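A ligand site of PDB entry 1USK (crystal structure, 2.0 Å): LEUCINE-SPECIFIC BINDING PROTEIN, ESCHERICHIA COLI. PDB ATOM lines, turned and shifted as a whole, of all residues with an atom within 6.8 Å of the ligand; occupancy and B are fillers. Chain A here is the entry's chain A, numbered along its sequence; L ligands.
The backbone NH (N) of Thr 102 lies within hydrogen-bond range of the side-chain hydroxyl (OG) of Ser 79, 3.4 Å away.
The backbone NH of Asn 103 sits at hydrogen-bond distance from the side-chain hydroxyl of Ser 79 (3.1 Å).
The backbone carbonyl oxygen of Ser 79 lies within hydrogen-bond range of the side-chain amide nitrogen of Gln 149 (3.4 Å).
The side-chain hydroxyl of Tyr 150 sits at hydrogen-bond distance from the side-chain carboxylate of Glu 226, at 2.5 Å.
NE2 of Gln 124 lies within hydrogen-bond range of OE1 of Glu 226.
The backbone NH (N) of Gly 227 is in hydrogen-bond range of the side-chain hydroxyl (OH) of Tyr 150, at 3.0 Å.
The side-chain sulfur (SG) of Cys 53 is disulfide-bonded to the side-chain sulfur (SG) of Cys 78 (2.1 Å).
O of Ala 101 sits at hydrogen-bond distance from NH1 of Arg 116 (2.9 Å).
An oxygen (O2) of the ligand sits at hydrogen-bond distance from the backbone NH (N) of Ser 79 (3.1 Å).
The side-chain hydroxyl of Ser 79 is in hydrogen-bond range of an oxygen (O1) of the ligand (2.5 Å).
The side-chain hydroxyl of Tyr 202 lies within hydrogen-bond range of an oxygen (O2) of the ligand (2.6 Å).
The backbone NH of Thr 102 sits at hydrogen-bond distance from an oxygen (O1) of the ligand, 3.2 Å away.
The side-chain hydroxyl of Thr 102 is in hydrogen-bond range of a nitrogen (N1) of the ligand.
A nitrogen (N1) of the ligand is in salt-bridge range of the side-chain carboxylate (OE2) of Glu 226.
The backbone carbonyl oxygen of Gly 100 is in hydrogen-bond range of a nitrogen (N1) of the ligand, 2.9 Å away.
Trp 18 touches the ligand (NE1 to C6, 3.8 Å).
O of Leu 77 touches C3 of the ligand (3.9 Å).
Cys 78 touches the ligand (CA to O2, 3.4 Å).
Ala 101 touches the ligand (CA to O1, 3.5 Å).
Tyr 150 touches the ligand.
Gly 227 touches the ligand.
Tyr 276 touches the ligand (CE2 to C5, 3.6 Å).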
ATOM      1  N   ILE A  15      -8.749 -11.088 -18.403  1.00  0.00           N
ATOM      2  CA  ILE A  15      -8.468 -11.987 -19.530  1.00  0.00           C
ATOM      3  C   ILE A  15      -8.878 -11.366 -20.861  1.00  0.00           C
ATOM      4  O   ILE A  15      -9.404 -12.028 -21.756  1.00  0.00           O
ATOM      5  CB  ILE A  15      -9.101 -13.386 -19.300  1.00  0.00           C
ATOM      6  CG1 ILE A  15     -10.610 -13.312 -19.141  1.00  0.00           C
ATOM      7  CG2 ILE A  15      -8.475 -14.049 -18.068  1.00  0.00           C
ATOM      8  CD1 ILE A  15     -11.297 -14.643 -19.376  1.00  0.00           C
ATOM      9  N   TRP A  18      -7.558 -12.835 -24.387  1.00  0.00           N
ATOM     10  CA  TRP A  18      -8.372 -13.793 -25.121  1.00  0.00           C
ATOM     11  C   TRP A  18      -9.336 -13.056 -26.036  1.00  0.00           C
ATOM     12  O   TRP A  18      -9.469 -13.395 -27.209  1.00  0.00           O
ATOM     13  CB  TRP A  18      -9.128 -14.738 -24.194  1.00  0.00           C
ATOM     14  CG  TRP A  18      -8.245 -15.776 -23.582  1.00  0.00           C
ATOM     15  CD1 TRP A  18      -8.126 -16.044 -22.250  1.00  0.00           C
ATOM     16  CD2 TRP A  18      -7.375 -16.690 -24.260  1.00  0.00           C
ATOM     17  NE1 TRP A  18      -7.232 -17.074 -22.065  1.00  0.00           N
ATOM     18  CE2 TRP A  18      -6.752 -17.486 -23.275  1.00  0.00           C
ATOM     19  CE3 TRP A  18      -7.043 -16.916 -25.613  1.00  0.00           C
ATOM     20  CZ2 TRP A  18      -5.828 -18.489 -23.589  1.00  0.00           C
ATOM     21  CZ3 TRP A  18      -6.121 -17.917 -25.918  1.00  0.00           C
ATOM     22  CH2 TRP A  18      -5.527 -18.687 -24.912  1.00  0.00           C
ATOM     23  N   GLY A  19      -9.998 -12.039 -25.488  1.00  0.00           N
ATOM     24  CA  GLY A  19     -10.906 -11.204 -26.263  1.00  0.00           C
ATOM     25  C   GLY A  19     -10.246 -10.538 -27.448  1.00  0.00           C
ATOM     26  O   GLY A  19     -10.868 -10.387 -28.483  1.00  0.00           O
ATOM     27  N   CYS A  53     -16.153 -10.575 -19.808  1.00  0.00           N
ATOM     28  CA  CYS A  53     -16.225 -11.951 -19.311  1.00  0.00           C
ATOM     29  C   CYS A  53     -16.743 -12.017 -17.869  1.00  0.00           C
ATOM     30  O   CYS A  53     -16.152 -12.656 -17.005  1.00  0.00           O
ATOM     31  CB  CYS A  53     -14.865 -12.641 -19.475  1.00  0.00           C
ATOM     32  SG  CYS A  53     -14.675 -13.467 -21.085  1.00  0.00           S
ATOM     33  N   LEU A  77     -17.658 -14.923 -25.002  1.00  0.00           N
ATOM     34  CA  LEU A  77     -16.339 -15.547 -25.012  1.00  0.00           C
ATOM     35  C   LEU A  77     -16.182 -16.629 -23.937  1.00  0.00           C
ATOM     36  O   LEU A  77     -15.837 -17.764 -24.241  1.00  0.00           O
ATOM     37  CB  LEU A  77     -15.262 -14.475 -24.826  1.00  0.00           C
ATOM     38  CG  LEU A  77     -13.794 -14.905 -24.976  1.00  0.00           C
ATOM     39  CD1 LEU A  77     -13.529 -15.532 -26.337  1.00  0.00           C
ATOM     40  CD2 LEU A  77     -12.888 -13.708 -24.760  1.00  0.00           C
ATOM     41  N   CYS A  78     -16.433 -16.262 -22.689  1.00  0.00           N
ATOM     42  CA  CYS A  78     -16.252 -17.175 -21.569  1.00  0.00           C
ATOM     43  C   CYS A  78     -17.526 -17.958 -21.303  1.00  0.00           C
ATOM     44  O   CYS A  78     -18.594 -17.568 -21.734  1.00  0.00           O
ATOM     45  CB  CYS A  78     -15.820 -16.382 -20.336  1.00  0.00           C
ATOM     46  SG  CYS A  78     -14.303 -15.437 -20.653  1.00  0.00           S
ATOM     47  N   SER A  79     -17.402 -19.069 -20.564  1.00  0.00           N
ATOM     48  CA  SER A  79     -18.537 -19.937 -20.281  1.00  0.00           C
ATOM     49  C   SER A  79     -19.517 -19.317 -19.287  1.00  0.00           C
ATOM     50  O   SER A  79     -20.732 -19.432 -19.464  1.00  0.00           O
ATOM     51  CB  SER A  79     -18.068 -21.278 -19.733  1.00  0.00           C
ATOM     52  OG  SER A  79     -17.427 -22.042 -20.743  1.00  0.00           O
ATOM     53  N   SER A  80     -18.985 -18.656 -18.266  1.00  0.00           N
ATOM     54  CA  SER A  80     -19.800 -18.072 -17.197  1.00  0.00           C
ATOM     55  C   SER A  80     -20.565 -16.830 -17.656  1.00  0.00           C
ATOM     56  O   SER A  80     -21.577 -16.487 -17.053  1.00  0.00           O
ATOM     57  CB  SER A  80     -18.929 -17.745 -15.981  1.00  0.00           C
ATOM     58  OG  SER A  80     -17.986 -16.725 -16.275  1.00  0.00           O
ATOM     59  N   PRO A  99     -17.876 -18.552 -30.041  1.00  0.00           N
ATOM     60  CA  PRO A  99     -16.539 -18.980 -30.461  1.00  0.00           C
ATOM     61  C   PRO A  99     -15.594 -19.343 -29.301  1.00  0.00           C
ATOM     62  O   PRO A  99     -14.500 -19.813 -29.578  1.00  0.00           O
ATOM     63  CB  PRO A  99     -16.005 -17.750 -31.191  1.00  0.00           C
ATOM     64  CG  PRO A  99     -16.618 -16.616 -30.457  1.00  0.00           C
ATOM     65  CD  PRO A  99     -17.971 -17.091 -29.987  1.00  0.00           C
ATOM     66  N   GLY A 100     -15.998 -19.149 -28.052  1.00  0.00           N
ATOM     67  CA  GLY A 100     -15.095 -19.320 -26.929  1.00  0.00           C
ATOM     68  C   GLY A 100     -15.507 -20.272 -25.809  1.00  0.00           C
ATOM     69  O   GLY A 100     -14.641 -20.906 -25.208  1.00  0.00           O
ATOM     70  N   ALA A 101     -16.801 -20.337 -25.512  1.00  0.00           N
ATOM     71  CA  ALA A 101     -17.313 -21.121 -24.386  1.00  0.00           C
ATOM     72  C   ALA A 101     -17.160 -22.603 -24.621  1.00  0.00           C
ATOM     73  O   ALA A 101     -17.675 -23.126 -25.614  1.00  0.00           O
ATOM     74  CB  ALA A 101     -18.784 -20.779 -24.125  1.00  0.00           C
ATOM     75  N   THR A 102     -16.453 -23.291 -23.722  1.00  0.00           N
ATOM     76  CA  THR A 102     -16.174 -24.722 -23.856  1.00  0.00           C
ATOM     77  C   THR A 102     -16.900 -25.592 -22.812  1.00  0.00           C
ATOM     78  O   THR A 102     -16.899 -26.818 -22.934  1.00  0.00           O
ATOM     79  CB  THR A 102     -14.644 -24.999 -23.740  1.00  0.00           C
ATOM     80  OG1 THR A 102     -14.101 -24.310 -22.607  1.00  0.00           O
ATOM     81  CG2 THR A 102     -13.877 -24.426 -24.924  1.00  0.00           C
ATOM     82  N   ASN A 103     -17.524 -24.980 -21.811  1.00  0.00           N
ATOM     83  CA  ASN A 103     -18.243 -25.733 -20.778  1.00  0.00           C
ATOM     84  C   ASN A 103     -19.461 -26.448 -21.369  1.00  0.00           C
ATOM     85  O   ASN A 103     -20.237 -25.810 -22.076  1.00  0.00           O
ATOM     86  CB  ASN A 103     -18.675 -24.809 -19.639  1.00  0.00           C
ATOM     87  CG  ASN A 103     -19.278 -25.569 -18.475  1.00  0.00           C
ATOM     88  OD1 ASN A 103     -20.499 -25.662 -18.344  1.00  0.00           O
ATOM     89  ND2 ASN A 103     -18.412 -26.124 -17.618  1.00  0.00           N
ATOM     90  N   ARG A 116     -22.019 -23.468 -31.163  1.00  0.00           N
ATOM     91  CA  ARG A 116     -20.660 -22.990 -30.881  1.00  0.00           C
ATOM     92  C   ARG A 116     -19.634 -23.573 -31.861  1.00  0.00           C
ATOM     93  O   ARG A 116     -19.839 -24.657 -32.402  1.00  0.00           O
ATOM     94  CB  ARG A 116     -20.261 -23.320 -29.442  1.00  0.00           C
ATOM     95  CG  ARG A 116     -20.118 -24.800 -29.128  1.00  0.00           C
ATOM     96  CD  ARG A 116     -19.642 -25.067 -27.705  1.00  0.00           C
ATOM     97  NE  ARG A 116     -20.640 -25.734 -26.857  1.00  0.00           N
ATOM     98  CZ  ARG A 116     -20.562 -25.819 -25.539  1.00  0.00           C
ATOM     99  NH1 ARG A 116     -19.549 -25.246 -24.883  1.00  0.00           N
ATOM    100  NH2 ARG A 116     -21.503 -26.450 -24.863  1.00  0.00           N
ATOM    101  N   ALA A 118     -16.371 -23.452 -30.623  1.00  0.00           N
ATOM    102  CA  ALA A 118     -15.375 -23.856 -29.651  1.00  0.00           C
ATOM    103  C   ALA A 118     -15.555 -25.333 -29.347  1.00  0.00           C
ATOM    104  O   ALA A 118     -16.585 -25.922 -29.680  1.00  0.00           O
ATOM    105  CB  ALA A 118     -15.511 -23.022 -28.386  1.00  0.00           C
ATOM    106  N   ASP A 121     -15.331 -29.105 -23.007  1.00  0.00           N
ATOM    107  CA  ASP A 121     -14.480 -29.485 -21.896  1.00  0.00           C
ATOM    108  C   ASP A 121     -14.745 -30.963 -21.537  1.00  0.00           C
ATOM    109  O   ASP A 121     -13.931 -31.615 -20.902  1.00  0.00           O
ATOM    110  CB  ASP A 121     -14.682 -28.561 -20.694  1.00  0.00           C
ATOM    111  CG  ASP A 121     -14.164 -27.134 -20.955  1.00  0.00           C
ATOM    112  OD1 ASP A 121     -13.157 -26.980 -21.699  1.00  0.00           O
ATOM    113  OD2 ASP A 121     -14.683 -26.111 -20.460  1.00  0.00           O
ATOM    114  N   GLN A 124     -11.808 -32.020 -23.436  1.00  0.00           N
ATOM    115  CA  GLN A 124     -10.540 -31.443 -23.016  1.00  0.00           C
ATOM    116  C   GLN A 124     -10.081 -32.019 -21.672  1.00  0.00           C
ATOM    117  O   GLN A 124      -8.896 -32.275 -21.470  1.00  0.00           O
ATOM    118  CB  GLN A 124     -10.628 -29.917 -22.931  1.00  0.00           C
ATOM    119  CG  GLN A 124      -9.420 -29.265 -22.247  1.00  0.00           C
ATOM    120  CD  GLN A 124      -9.148 -27.845 -22.707  1.00  0.00           C
ATOM    121  OE1 GLN A 124      -8.015 -27.513 -23.063  1.00  0.00           O
ATOM    122  NE2 GLN A 124     -10.171 -26.990 -22.678  1.00  0.00           N
ATOM    123  N   GLN A 149     -17.107 -21.278 -13.579  1.00  0.00           N
ATOM    124  CA  GLN A 149     -17.724 -22.372 -14.335  1.00  0.00           C
ATOM    125  C   GLN A 149     -16.748 -23.146 -15.237  1.00  0.00           C
ATOM    126  O   GLN A 149     -16.796 -24.365 -15.298  1.00  0.00           O
ATOM    127  CB  GLN A 149     -18.908 -21.845 -15.154  1.00  0.00           C
ATOM    128  CG  GLN A 149     -19.856 -22.947 -15.617  1.00  0.00           C
ATOM    129  CD  GLN A 149     -21.177 -22.433 -16.192  1.00  0.00           C
ATOM    130  OE1 GLN A 149     -22.122 -23.198 -16.346  1.00  0.00           O
ATOM    131  NE2 GLN A 149     -21.230 -21.150 -16.521  1.00  0.00           N
ATOM    132  N   TYR A 150     -15.864 -22.424 -15.933  1.00  0.00           N
ATOM    133  CA  TYR A 150     -14.904 -23.059 -16.845  1.00  0.00           C
ATOM    134  C   TYR A 150     -13.832 -23.851 -16.104  1.00  0.00           C
ATOM    135  O   TYR A 150     -13.628 -25.030 -16.378  1.00  0.00           O
ATOM    136  CB  TYR A 150     -14.282 -21.984 -17.744  1.00  0.00           C
ATOM    137  CG  TYR A 150     -13.043 -22.413 -18.508  1.00  0.00           C
ATOM    138  CD1 TYR A 150     -13.152 -23.170 -19.677  1.00  0.00           C
ATOM    139  CD2 TYR A 150     -11.773 -22.046 -18.088  1.00  0.00           C
ATOM    140  CE1 TYR A 150     -12.025 -23.553 -20.382  1.00  0.00           C
ATOM    141  CE2 TYR A 150     -10.642 -22.420 -18.794  1.00  0.00           C
ATOM    142  CZ  TYR A 150     -10.777 -23.175 -19.948  1.00  0.00           C
ATOM    143  OH  TYR A 150      -9.678 -23.567 -20.647  1.00  0.00           O
ATOM    144  N   GLY A 151     -13.165 -23.214 -15.152  1.00  0.00           N
ATOM    145  CA  GLY A 151     -12.056 -23.839 -14.446  1.00  0.00           C
ATOM    146  C   GLY A 151     -12.467 -24.952 -13.513  1.00  0.00           C
ATOM    147  O   GLY A 151     -11.855 -26.024 -13.498  1.00  0.00           O
ATOM    148  N   LEU A 154     -13.613 -28.083 -15.477  1.00  0.00           N
ATOM    149  CA  LEU A 154     -12.470 -28.852 -15.998  1.00  0.00           C
ATOM    150  C   LEU A 154     -11.704 -29.556 -14.872  1.00  0.00           C
ATOM    151  O   LEU A 154     -11.144 -30.626 -15.088  1.00  0.00           O
ATOM    152  CB  LEU A 154     -11.515 -27.951 -16.787  1.00  0.00           C
ATOM    153  CG  LEU A 154     -11.847 -27.753 -18.257  1.00  0.00           C
ATOM    154  CD1 LEU A 154     -11.336 -26.401 -18.745  1.00  0.00           C
ATOM    155  CD2 LEU A 154     -11.281 -28.887 -19.096  1.00  0.00           C
ATOM    156  N   GLY A 201      -8.507 -23.166 -14.839  1.00  0.00           N
ATOM    157  CA  GLY A 201      -8.548 -21.712 -14.823  1.00  0.00           C
ATOM    158  C   GLY A 201      -7.844 -21.030 -15.980  1.00  0.00           C
ATOM    159  O   GLY A 201      -7.548 -21.639 -17.014  1.00  0.00           O
ATOM    160  N   TYR A 202      -7.569 -19.748 -15.797  1.00  0.00           N
ATOM    161  CA  TYR A 202      -7.013 -18.898 -16.832  1.00  0.00           C
ATOM    162  C   TYR A 202      -5.564 -18.489 -16.495  1.00  0.00           C
ATOM    163  O   TYR A 202      -5.071 -18.762 -15.391  1.00  0.00           O
ATOM    164  CB  TYR A 202      -7.886 -17.658 -17.013  1.00  0.00           C
ATOM    165  CG  TYR A 202      -9.344 -17.952 -17.343  1.00  0.00           C
ATOM    166  CD1 TYR A 202      -9.707 -18.521 -18.564  1.00  0.00           C
ATOM    167  CD2 TYR A 202     -10.361 -17.644 -16.442  1.00  0.00           C
ATOM    168  CE1 TYR A 202     -11.040 -18.772 -18.876  1.00  0.00           C
ATOM    169  CE2 TYR A 202     -11.696 -17.893 -16.744  1.00  0.00           C
ATOM    170  CZ  TYR A 202     -12.039 -18.459 -17.951  1.00  0.00           C
ATOM    171  OH  TYR A 202     -13.358 -18.713 -18.237  1.00  0.00           O
ATOM    172  N   GLU A 226      -6.683 -24.897 -22.010  1.00  0.00           N
ATOM    173  CA  GLU A 226      -6.274 -23.936 -23.037  1.00  0.00           C
ATOM    174  C   GLU A 226      -6.341 -22.481 -22.568  1.00  0.00           C
ATOM    175  O   GLU A 226      -5.689 -21.609 -23.148  1.00  0.00           O
ATOM    176  CB  GLU A 226      -7.058 -24.136 -24.363  1.00  0.00           C
ATOM    177  CG  GLU A 226      -8.181 -23.146 -24.664  1.00  0.00           C
ATOM    178  CD  GLU A 226      -9.445 -23.374 -23.848  1.00  0.00           C
ATOM    179  OE1 GLU A 226      -9.519 -24.335 -23.069  1.00  0.00           O
ATOM    180  OE2 GLU A 226     -10.390 -22.572 -23.999  1.00  0.00           O
ATOM    181  N   GLY A 227      -7.108 -22.239 -21.504  1.00  0.00           N
ATOM    182  CA  GLY A 227      -7.227 -20.934 -20.892  1.00  0.00           C
ATOM    183  C   GLY A 227      -5.957 -20.364 -20.303  1.00  0.00           C
ATOM    184  O   GLY A 227      -5.872 -19.148 -20.107  1.00  0.00           O
ATOM    185  N   VAL A 228      -4.979 -21.210 -19.989  1.00  0.00           N
ATOM    186  CA  VAL A 228      -3.666 -20.738 -19.528  1.00  0.00           C
ATOM    187  C   VAL A 228      -2.654 -20.569 -20.671  1.00  0.00           C
ATOM    188  O   VAL A 228      -1.637 -19.900 -20.482  1.00  0.00           O
ATOM    189  CB  VAL A 228      -3.065 -21.655 -18.419  1.00  0.00           C
ATOM    190  CG1 VAL A 228      -4.097 -21.920 -17.345  1.00  0.00           C
ATOM    191  CG2 VAL A 228      -2.527 -22.960 -19.000  1.00  0.00           C
ATOM    192  N   TYR A 276      -8.180 -18.819 -30.709  1.00  0.00           N
ATOM    193  CA  TYR A 276      -9.484 -18.161 -30.850  1.00  0.00           C
ATOM    194  C   TYR A 276      -9.562 -17.069 -31.908  1.00  0.00           C
ATOM    195  O   TYR A 276     -10.641 -16.573 -32.196  1.00  0.00           O
ATOM    196  CB  TYR A 276      -9.967 -17.666 -29.480  1.00  0.00           C
ATOM    197  CG  TYR A 276     -10.287 -18.823 -28.571  1.00  0.00           C
ATOM    198  CD1 TYR A 276     -11.418 -19.598 -28.796  1.00  0.00           C
ATOM    199  CD2 TYR A 276      -9.431 -19.190 -27.534  1.00  0.00           C
ATOM    200  CE1 TYR A 276     -11.718 -20.674 -27.992  1.00  0.00           C
ATOM    201  CE2 TYR A 276      -9.728 -20.278 -26.717  1.00  0.00           C
ATOM    202  CZ  TYR A 276     -10.877 -21.024 -26.951  1.00  0.00           C
ATOM    203  OH  TYR A 276     -11.203 -22.102 -26.174  1.00  0.00           O
HETATM  204  N1  LIG L   1     -12.938 -21.849 -23.053  1.00  0.00           N
HETATM  205  C1  LIG L   1     -12.907 -20.756 -22.084  1.00  0.00           C
HETATM  206  C2  LIG L   1     -14.222 -20.634 -21.317  1.00  0.00           C
HETATM  207  O1  LIG L   1     -15.190 -21.364 -21.566  1.00  0.00           O
HETATM  208  C3  LIG L   1     -12.613 -19.423 -22.773  1.00  0.00           C
HETATM  209  C4  LIG L   1     -11.303 -19.356 -23.557  1.00  0.00           C
HETATM  210  C5  LIG L   1     -11.251 -18.067 -24.365  1.00  0.00           C
HETATM  211  C6  LIG L   1     -10.103 -19.450 -22.633  1.00  0.00           C
HETATM  212  O2  LIG L   1     -14.366 -19.800 -20.429  1.00  0.00           O
